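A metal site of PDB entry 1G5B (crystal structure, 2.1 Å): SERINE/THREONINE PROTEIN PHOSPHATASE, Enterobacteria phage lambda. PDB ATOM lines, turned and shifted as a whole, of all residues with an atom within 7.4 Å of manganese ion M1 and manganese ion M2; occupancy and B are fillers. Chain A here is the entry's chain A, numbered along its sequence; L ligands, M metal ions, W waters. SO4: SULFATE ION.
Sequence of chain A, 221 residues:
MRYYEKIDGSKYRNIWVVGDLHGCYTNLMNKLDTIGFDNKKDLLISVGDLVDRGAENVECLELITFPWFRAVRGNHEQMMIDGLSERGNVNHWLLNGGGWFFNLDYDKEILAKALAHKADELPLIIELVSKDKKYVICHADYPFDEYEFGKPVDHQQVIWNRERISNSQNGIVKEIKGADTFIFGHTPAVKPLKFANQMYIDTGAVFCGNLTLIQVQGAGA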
ATOM      1  N   GLY A  19     -15.460   2.328  -0.297  1.00  0.00           N
ATOM      2  CA  GLY A  19     -14.696   1.459  -1.188  1.00  0.00           C
ATOM      3  C   GLY A  19     -14.754   1.922  -2.637  1.00  0.00           C
ATOM      4  O   GLY A  19     -15.300   2.979  -2.945  1.00  0.00           O
ATOM      5  N   ASP A  20     -14.178   1.124  -3.540  1.00  0.00           N
ATOM      6  CA  ASP A  20     -14.131   1.445  -4.970  1.00  0.00           C
ATOM      7  C   ASP A  20     -15.470   1.920  -5.515  1.00  0.00           C
ATOM      8  O   ASP A  20     -16.482   1.231  -5.371  1.00  0.00           O
ATOM      9  CB  ASP A  20     -13.637   0.210  -5.744  1.00  0.00           C
ATOM     10  CG  ASP A  20     -12.298  -0.287  -5.247  1.00  0.00           C
ATOM     11  OD1 ASP A  20     -12.153  -0.417  -4.016  1.00  0.00           O
ATOM     12  OD2 ASP A  20     -11.390  -0.555  -6.071  1.00  0.00           O
ATOM     13  N   LEU A  21     -15.466   3.096  -6.126  1.00  0.00           N
ATOM     14  CA  LEU A  21     -16.696   3.676  -6.673  1.00  0.00           C
ATOM     15  C   LEU A  21     -17.006   3.342  -8.133  1.00  0.00           C
ATOM     16  O   LEU A  21     -18.173   3.127  -8.475  1.00  0.00           O
ATOM     17  CB  LEU A  21     -16.654   5.196  -6.502  1.00  0.00           C
ATOM     18  CG  LEU A  21     -16.896   5.649  -5.057  1.00  0.00           C
ATOM     19  CD1 LEU A  21     -16.572   7.130  -4.904  1.00  0.00           C
ATOM     20  CD2 LEU A  21     -18.361   5.366  -4.695  1.00  0.00           C
ATOM     21  N   HIS A  22     -15.983   3.325  -8.979  1.00  0.00           N
ATOM     22  CA  HIS A  22     -16.153   3.015 -10.393  1.00  0.00           C
ATOM     23  C   HIS A  22     -17.438   3.568 -11.003  1.00  0.00           C
ATOM     24  O   HIS A  22     -18.291   2.816 -11.467  1.00  0.00           O
ATOM     25  CB  HIS A  22     -16.101   1.506 -10.619  1.00  0.00           C
ATOM     26  CG  HIS A  22     -14.766   0.897 -10.335  1.00  0.00           C
ATOM     27  ND1 HIS A  22     -13.624   1.253 -11.018  1.00  0.00           N
ATOM     28  CD2 HIS A  22     -14.379  -0.042  -9.433  1.00  0.00           C
ATOM     29  CE1 HIS A  22     -12.596   0.563 -10.554  1.00  0.00           C
ATOM     30  NE2 HIS A  22     -13.031  -0.220  -9.585  1.00  0.00           N
ATOM     31  N   VAL A  47     -10.881   5.250  -1.113  1.00  0.00           N
ATOM     32  CA  VAL A  47      -9.739   4.379  -1.400  1.00  0.00           C
ATOM     33  C   VAL A  47      -9.308   4.459  -2.859  1.00  0.00           C
ATOM     34  O   VAL A  47      -8.376   3.776  -3.278  1.00  0.00           O
ATOM     35  CB  VAL A  47     -10.063   2.899  -1.072  1.00  0.00           C
ATOM     36  CG1 VAL A  47     -10.458   2.754   0.383  1.00  0.00           C
ATOM     37  CG2 VAL A  47     -11.175   2.389  -1.995  1.00  0.00           C
ATOM     38  N   GLY A  48      -9.979   5.285  -3.651  1.00  0.00           N
ATOM     39  CA  GLY A  48      -9.613   5.397  -5.043  1.00  0.00           C
ATOM     40  C   GLY A  48     -10.454   4.548  -5.975  1.00  0.00           C
ATOM     41  O   GLY A  48     -11.441   3.932  -5.547  1.00  0.00           O
ATOM     42  N   ASP A  49     -10.052   4.486  -7.252  1.00  0.00           N
ATOM     43  CA  ASP A  49     -10.780   3.753  -8.282  1.00  0.00           C
ATOM     44  C   ASP A  49     -12.156   4.367  -8.420  1.00  0.00           C
ATOM     45  O   ASP A  49     -13.199   3.724  -8.262  1.00  0.00           O
ATOM     46  CB  ASP A  49     -10.881   2.254  -7.930  1.00  0.00           C
ATOM     47  CG  ASP A  49      -9.756   1.437  -8.546  1.00  0.00           C
ATOM     48  OD1 ASP A  49      -8.754   2.048  -9.001  1.00  0.00           O
ATOM     49  OD2 ASP A  49      -9.853   0.203  -8.569  1.00  0.00           O
ATOM     50  N   LEU A  50     -12.140   5.662  -8.716  1.00  0.00           N
ATOM     51  CA  LEU A  50     -13.351   6.463  -8.877  1.00  0.00           C
ATOM     52  C   LEU A  50     -13.984   6.276 -10.255  1.00  0.00           C
ATOM     53  O   LEU A  50     -15.198   6.460 -10.407  1.00  0.00           O
ATOM     54  CB  LEU A  50     -13.009   7.943  -8.706  1.00  0.00           C
ATOM     55  CG  LEU A  50     -12.226   8.373  -7.450  1.00  0.00           C
ATOM     56  CD1 LEU A  50     -11.901   9.848  -7.535  1.00  0.00           C
ATOM     57  CD2 LEU A  50     -13.050   8.085  -6.203  1.00  0.00           C
ATOM     58  N   VAL A  51     -13.178   5.902 -11.235  1.00  0.00           N
ATOM     59  CA  VAL A  51     -13.669   5.746 -12.605  1.00  0.00           C
ATOM     60  C   VAL A  51     -13.473   4.374 -13.239  1.00  0.00           C
ATOM     61  O   VAL A  51     -12.838   3.480 -12.668  1.00  0.00           O
ATOM     62  CB  VAL A  51     -13.021   6.796 -13.503  1.00  0.00           C
ATOM     63  CG1 VAL A  51     -13.369   8.196 -13.022  1.00  0.00           C
ATOM     64  CG2 VAL A  51     -11.504   6.613 -13.518  1.00  0.00           C
ATOM     65  N   ASP A  52     -14.027   4.233 -14.441  1.00  0.00           N
ATOM     66  CA  ASP A  52     -13.959   3.016 -15.255  1.00  0.00           C
ATOM     67  C   ASP A  52     -15.018   1.960 -14.946  1.00  0.00           C
ATOM     68  O   ASP A  52     -15.423   1.795 -13.794  1.00  0.00           O
ATOM     69  CB  ASP A  52     -12.579   2.366 -15.145  1.00  0.00           C
ATOM     70  CG  ASP A  52     -11.463   3.249 -15.678  1.00  0.00           C
ATOM     71  OD1 ASP A  52     -11.751   4.248 -16.370  1.00  0.00           O
ATOM     72  OD2 ASP A  52     -10.289   2.922 -15.415  1.00  0.00           O
ATOM     73  N   GLY A  74      -6.201   5.473  -7.107  1.00  0.00           N
ATOM     74  CA  GLY A  74      -6.271   4.033  -7.289  1.00  0.00           C
ATOM     75  C   GLY A  74      -5.529   3.665  -8.568  1.00  0.00           C
ATOM     76  O   GLY A  74      -5.085   4.560  -9.288  1.00  0.00           O
ATOM     77  N   ASN A  75      -5.383   2.376  -8.866  1.00  0.00           N
ATOM     78  CA  ASN A  75      -4.679   2.011 -10.090  1.00  0.00           C
ATOM     79  C   ASN A  75      -5.440   2.476 -11.340  1.00  0.00           C
ATOM     80  O   ASN A  75      -4.847   2.711 -12.395  1.00  0.00           O
ATOM     81  CB  ASN A  75      -4.366   0.496 -10.138  1.00  0.00           C
ATOM     82  CG  ASN A  75      -5.597  -0.405 -10.116  1.00  0.00           C
ATOM     83  OD1 ASN A  75      -6.448  -0.311  -9.226  1.00  0.00           O
ATOM     84  ND2 ASN A  75      -5.690  -1.304 -11.095  1.00  0.00           N
ATOM     85  N   HIS A  76      -6.758   2.663 -11.217  1.00  0.00           N
ATOM     86  CA  HIS A  76      -7.521   3.133 -12.355  1.00  0.00           C
ATOM     87  C   HIS A  76      -7.224   4.608 -12.610  1.00  0.00           C
ATOM     88  O   HIS A  76      -7.138   5.030 -13.764  1.00  0.00           O
ATOM     89  CB  HIS A  76      -9.017   2.875 -12.130  1.00  0.00           C
ATOM     90  CG  HIS A  76      -9.418   1.461 -12.430  1.00  0.00           C
ATOM     91  ND1 HIS A  76     -10.048   1.091 -13.596  1.00  0.00           N
ATOM     92  CD2 HIS A  76      -9.204   0.309 -11.737  1.00  0.00           C
ATOM     93  CE1 HIS A  76     -10.188  -0.214 -13.623  1.00  0.00           C
ATOM     94  NE2 HIS A  76      -9.682  -0.717 -12.506  1.00  0.00           N
ATOM     95  N   GLU A  77      -7.069   5.402 -11.551  1.00  0.00           N
ATOM     96  CA  GLU A  77      -6.743   6.814 -11.755  1.00  0.00           C
ATOM     97  C   GLU A  77      -5.379   6.879 -12.450  1.00  0.00           C
ATOM     98  O   GLU A  77      -5.165   7.676 -13.370  1.00  0.00           O
ATOM     99  CB  GLU A  77      -6.658   7.576 -10.429  1.00  0.00           C
ATOM    100  CG  GLU A  77      -7.993   8.064  -9.900  1.00  0.00           C
ATOM    101  CD  GLU A  77      -8.884   6.942  -9.402  1.00  0.00           C
ATOM    102  OE1 GLU A  77     -10.104   7.005  -9.649  1.00  0.00           O
ATOM    103  OE2 GLU A  77      -8.364   6.018  -8.751  1.00  0.00           O
ATOM    104  N   MET A  79      -3.975   4.626 -14.436  1.00  0.00           N
ATOM    105  CA  MET A  79      -4.070   4.202 -15.841  1.00  0.00           C
ATOM    106  C   MET A  79      -4.673   5.319 -16.688  1.00  0.00           C
ATOM    107  O   MET A  79      -4.266   5.525 -17.835  1.00  0.00           O
ATOM    108  CB  MET A  79      -4.918   2.928 -15.982  1.00  0.00           C
ATOM    109  CG  MET A  79      -4.222   1.671 -15.454  1.00  0.00           C
ATOM    110  SD  MET A  79      -5.132   0.153 -15.846  1.00  0.00           S
ATOM    111  CE  MET A  79      -6.134  -0.011 -14.370  1.00  0.00           C
ATOM    112  N   HIS A 139      -5.012   2.339  -1.675  1.00  0.00           N
ATOM    113  CA  HIS A 139      -5.932   1.661  -2.562  1.00  0.00           C
ATOM    114  C   HIS A 139      -5.845   0.134  -2.482  1.00  0.00           C
ATOM    115  O   HIS A 139      -6.846  -0.540  -2.250  1.00  0.00           O
ATOM    116  CB  HIS A 139      -5.725   2.075  -4.018  1.00  0.00           C
ATOM    117  CG  HIS A 139      -6.640   1.367  -4.970  1.00  0.00           C
ATOM    118  ND1 HIS A 139      -8.014   1.476  -4.886  1.00  0.00           N
ATOM    119  CD2 HIS A 139      -6.389   0.468  -5.943  1.00  0.00           C
ATOM    120  CE1 HIS A 139      -8.577   0.671  -5.773  1.00  0.00           C
ATOM    121  NE2 HIS A 139      -7.608   0.045  -6.424  1.00  0.00           N
ATOM    122  N   ALA A 140      -4.650  -0.421  -2.669  1.00  0.00           N
ATOM    123  CA  ALA A 140      -4.491  -1.871  -2.636  1.00  0.00           C
ATOM    124  C   ALA A 140      -3.751  -2.404  -1.419  1.00  0.00           C
ATOM    125  O   ALA A 140      -4.151  -3.422  -0.846  1.00  0.00           O
ATOM    126  CB  ALA A 140      -3.775  -2.355  -3.916  1.00  0.00           C
ATOM    127  N   ILE A 159      -0.865   0.516  -5.208  1.00  0.00           N
ATOM    128  CA  ILE A 159      -2.121   0.471  -5.955  1.00  0.00           C
ATOM    129  C   ILE A 159      -2.444  -0.795  -6.747  1.00  0.00           C
ATOM    130  O   ILE A 159      -3.570  -0.931  -7.239  1.00  0.00           O
ATOM    131  CB  ILE A 159      -2.223   1.684  -6.916  1.00  0.00           C
ATOM    132  CG1 ILE A 159      -1.128   1.607  -7.976  1.00  0.00           C
ATOM    133  CG2 ILE A 159      -2.098   2.978  -6.109  1.00  0.00           C
ATOM    134  CD1 ILE A 159      -1.199   2.741  -8.993  1.00  0.00           C
ATOM    135  N   TRP A 160      -1.495  -1.720  -6.876  1.00  0.00           N
ATOM    136  CA  TRP A 160      -1.762  -2.963  -7.614  1.00  0.00           C
ATOM    137  C   TRP A 160      -1.647  -4.255  -6.808  1.00  0.00           C
ATOM    138  O   TRP A 160      -2.386  -5.210  -7.027  1.00  0.00           O
ATOM    139  CB  TRP A 160      -0.844  -3.102  -8.839  1.00  0.00           C
ATOM    140  CG  TRP A 160      -1.226  -2.264 -10.014  1.00  0.00           C
ATOM    141  CD1 TRP A 160      -0.733  -1.034 -10.334  1.00  0.00           C
ATOM    142  CD2 TRP A 160      -2.160  -2.599 -11.053  1.00  0.00           C
ATOM    143  NE1 TRP A 160      -1.308  -0.585 -11.505  1.00  0.00           N
ATOM    144  CE2 TRP A 160      -2.183  -1.526 -11.958  1.00  0.00           C
ATOM    145  CE3 TRP A 160      -2.982  -3.717 -11.292  1.00  0.00           C
ATOM    146  CZ2 TRP A 160      -3.002  -1.524 -13.104  1.00  0.00           C
ATOM    147  CZ3 TRP A 160      -3.796  -3.717 -12.425  1.00  0.00           C
ATOM    148  CH2 TRP A 160      -3.794  -2.624 -13.320  1.00  0.00           C
ATOM    149  N   ARG A 162      -1.767  -7.480  -4.609  1.00  0.00           N
ATOM    150  CA  ARG A 162      -2.833  -8.290  -4.014  1.00  0.00           C
ATOM    151  C   ARG A 162      -2.198  -9.434  -3.224  1.00  0.00           C
ATOM    152  O   ARG A 162      -2.891 -10.315  -2.728  1.00  0.00           O
ATOM    153  CB  ARG A 162      -3.740  -8.868  -5.092  1.00  0.00           C
ATOM    154  CG  ARG A 162      -4.698  -7.879  -5.729  1.00  0.00           C
ATOM    155  CD  ARG A 162      -5.828  -8.619  -6.425  1.00  0.00           C
ATOM    156  NE  ARG A 162      -6.914  -7.736  -6.825  1.00  0.00           N
ATOM    157  CZ  ARG A 162      -6.963  -7.068  -7.976  1.00  0.00           C
ATOM    158  NH1 ARG A 162      -5.973  -7.185  -8.856  1.00  0.00           N
ATOM    159  NH2 ARG A 162      -7.995  -6.289  -8.242  1.00  0.00           N
ATOM    160  N   GLY A 185      -9.083  -1.076  -0.629  1.00  0.00           N
ATOM    161  CA  GLY A 185     -10.162  -1.431  -1.533  1.00  0.00           C
ATOM    162  C   GLY A 185      -9.486  -2.319  -2.558  1.00  0.00           C
ATOM    163  O   GLY A 185      -8.807  -3.269  -2.177  1.00  0.00           O
ATOM    164  N   HIS A 186      -9.675  -2.026  -3.844  1.00  0.00           N
ATOM    165  CA  HIS A 186      -9.026  -2.754  -4.929  1.00  0.00           C
ATOM    166  C   HIS A 186      -9.440  -4.216  -5.165  1.00  0.00           C
ATOM    167  O   HIS A 186      -9.764  -4.585  -6.292  1.00  0.00           O
ATOM    168  CB  HIS A 186      -7.506  -2.699  -4.744  1.00  0.00           C
ATOM    169  CG  HIS A 186      -6.722  -3.247  -5.903  1.00  0.00           C
ATOM    170  ND1 HIS A 186      -6.848  -2.762  -7.189  1.00  0.00           N
ATOM    171  CD2 HIS A 186      -5.768  -4.208  -5.956  1.00  0.00           C
ATOM    172  CE1 HIS A 186      -6.003  -3.400  -7.977  1.00  0.00           C
ATOM    173  NE2 HIS A 186      -5.330  -4.279  -7.252  1.00  0.00           N
ATOM    174  N   THR A 187      -9.433  -5.043  -4.127  1.00  0.00           N
ATOM    175  CA  THR A 187      -9.806  -6.445  -4.264  1.00  0.00           C
ATOM    176  C   THR A 187     -11.221  -6.688  -3.777  1.00  0.00           C
ATOM    177  O   THR A 187     -11.488  -6.671  -2.574  1.00  0.00           O
ATOM    178  CB  THR A 187      -8.829  -7.348  -3.487  1.00  0.00           C
ATOM    179  OG1 THR A 187      -7.498  -7.167  -3.994  1.00  0.00           O
ATOM    180  CG2 THR A 187      -9.215  -8.810  -3.635  1.00  0.00           C
ATOM    181  N   PRO A 188     -12.165  -6.912  -4.710  1.00  0.00           N
ATOM    182  CA  PRO A 188     -13.580  -7.154  -4.409  1.00  0.00           C
ATOM    183  C   PRO A 188     -13.839  -8.398  -3.572  1.00  0.00           C
ATOM    184  O   PRO A 188     -13.096  -9.377  -3.627  1.00  0.00           O
ATOM    185  CB  PRO A 188     -14.211  -7.274  -5.794  1.00  0.00           C
ATOM    186  CG  PRO A 188     -13.261  -6.536  -6.692  1.00  0.00           C
ATOM    187  CD  PRO A 188     -11.930  -6.963  -6.160  1.00  0.00           C
ATOM    188  N   ASP A 202     -13.952  -3.123  -0.506  1.00  0.00           N
ATOM    189  CA  ASP A 202     -14.406  -3.119  -1.881  1.00  0.00           C
ATOM    190  C   ASP A 202     -15.396  -4.272  -2.055  1.00  0.00           C
ATOM    191  O   ASP A 202     -14.990  -5.426  -2.194  1.00  0.00           O
ATOM    192  CB  ASP A 202     -13.238  -3.296  -2.848  1.00  0.00           C
ATOM    193  CG  ASP A 202     -13.687  -3.324  -4.309  1.00  0.00           C
ATOM    194  OD1 ASP A 202     -14.873  -3.041  -4.567  1.00  0.00           O
ATOM    195  OD2 ASP A 202     -12.849  -3.616  -5.191  1.00  0.00           O
ATOM    196  N   VAL A 206     -19.795  -1.525  -8.564  1.00  0.00           N
ATOM    197  CA  VAL A 206     -20.033  -1.432 -10.002  1.00  0.00           C
ATOM    198  C   VAL A 206     -20.639  -2.724 -10.562  1.00  0.00           C
ATOM    199  O   VAL A 206     -21.421  -2.687 -11.507  1.00  0.00           O
ATOM    200  CB  VAL A 206     -18.713  -1.108 -10.762  1.00  0.00           C
ATOM    201  CG1 VAL A 206     -17.769  -2.297 -10.702  1.00  0.00           C
ATOM    202  CG2 VAL A 206     -19.022  -0.748 -12.198  1.00  0.00           C
HETATM  203  S   SO4 L   1      -8.419  -3.594 -10.874  1.00  0.00           S
HETATM  204  O1  SO4 L   1      -9.077  -4.416  -9.833  1.00  0.00           O
HETATM  205  O2  SO4 L   1      -7.157  -4.233 -11.277  1.00  0.00           O
HETATM  206  O3  SO4 L   1      -8.139  -2.252 -10.327  1.00  0.00           O
HETATM  207  O4  SO4 L   1      -9.298  -3.483 -12.056  1.00  0.00           O
HETATM  208 MN    MN M   1      -8.046  -1.179  -8.177  1.00  0.00          MN
HETATM  209 MN    MN M   2     -11.527  -1.250  -8.352  1.00  0.00          MN
HETATM  210  O   HOH W   1      -9.885  -2.548  -8.110  1.00  0.00           O
HETATM  211  O   HOH W   2     -12.927  -2.959  -7.757  1.00  0.00           O
HETATM  212  O   HOH W   3     -11.529  -2.781 -10.513  1.00  0.00           O
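Within 4 Å of manganese ion M2: Asp 20, His 22 and Asp 49. The nearest printed residue that does not touch manganese ion M2 is Asp 202 (4.2 Å).
Four residues have an atom within 4 Å of manganese ion M1: Asp 49, Asn 75, His 139 and His 186.
N of Gly 185 sits at hydrogen-bond distance from O of His 139 (2.8 Å). ND1 of His 139 sits at hydrogen-bond distance from O of Val 47, 2.8 Å away. ND1 of His 22 is in hydrogen-bond range of O of Val 51. The backbone NH (N) of His 186 lies within hydrogen-bond range of the side-chain carboxylate (OD1) of Asp 20 (3.0 Å). The guanidinium group of Arg 162 sits at hydrogen-bond distance from the backbone carbonyl oxygen of His 186 (3.1 Å). NE2 of His 186 sits at hydrogen-bond distance from O of Trp 160 (3.1 Å). N of Leu 21 lies within hydrogen-bond range of O of Asp 49 (3.2 Å). The backbone NH (N) of Asp 49 lies within hydrogen-bond range of the side-chain carboxylate (OE2) of Glu 77.
Manganese ion M2 is bound by water W1 (2.1 Å), NE2 of His 22 (2.2 Å), OD2 of Asp 49 (2.2 Å), water W2 (2.3 Å), OD2 of Asp 20 (2.4 Å) and water W3 (2.6 Å). Manganese ion M2 has six donor atoms within binding distance.
Manganese ion M1 is bound by the side-chain amide oxygen of Asn 75, a ring nitrogen (NE2) of His 139, a ring nitrogen (ND1) of His 186, water W1, the side-chain carboxylate of Asp 49 and an oxygen (O3) of the ligand. Manganese ion M1 has six donor atoms within binding distance.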
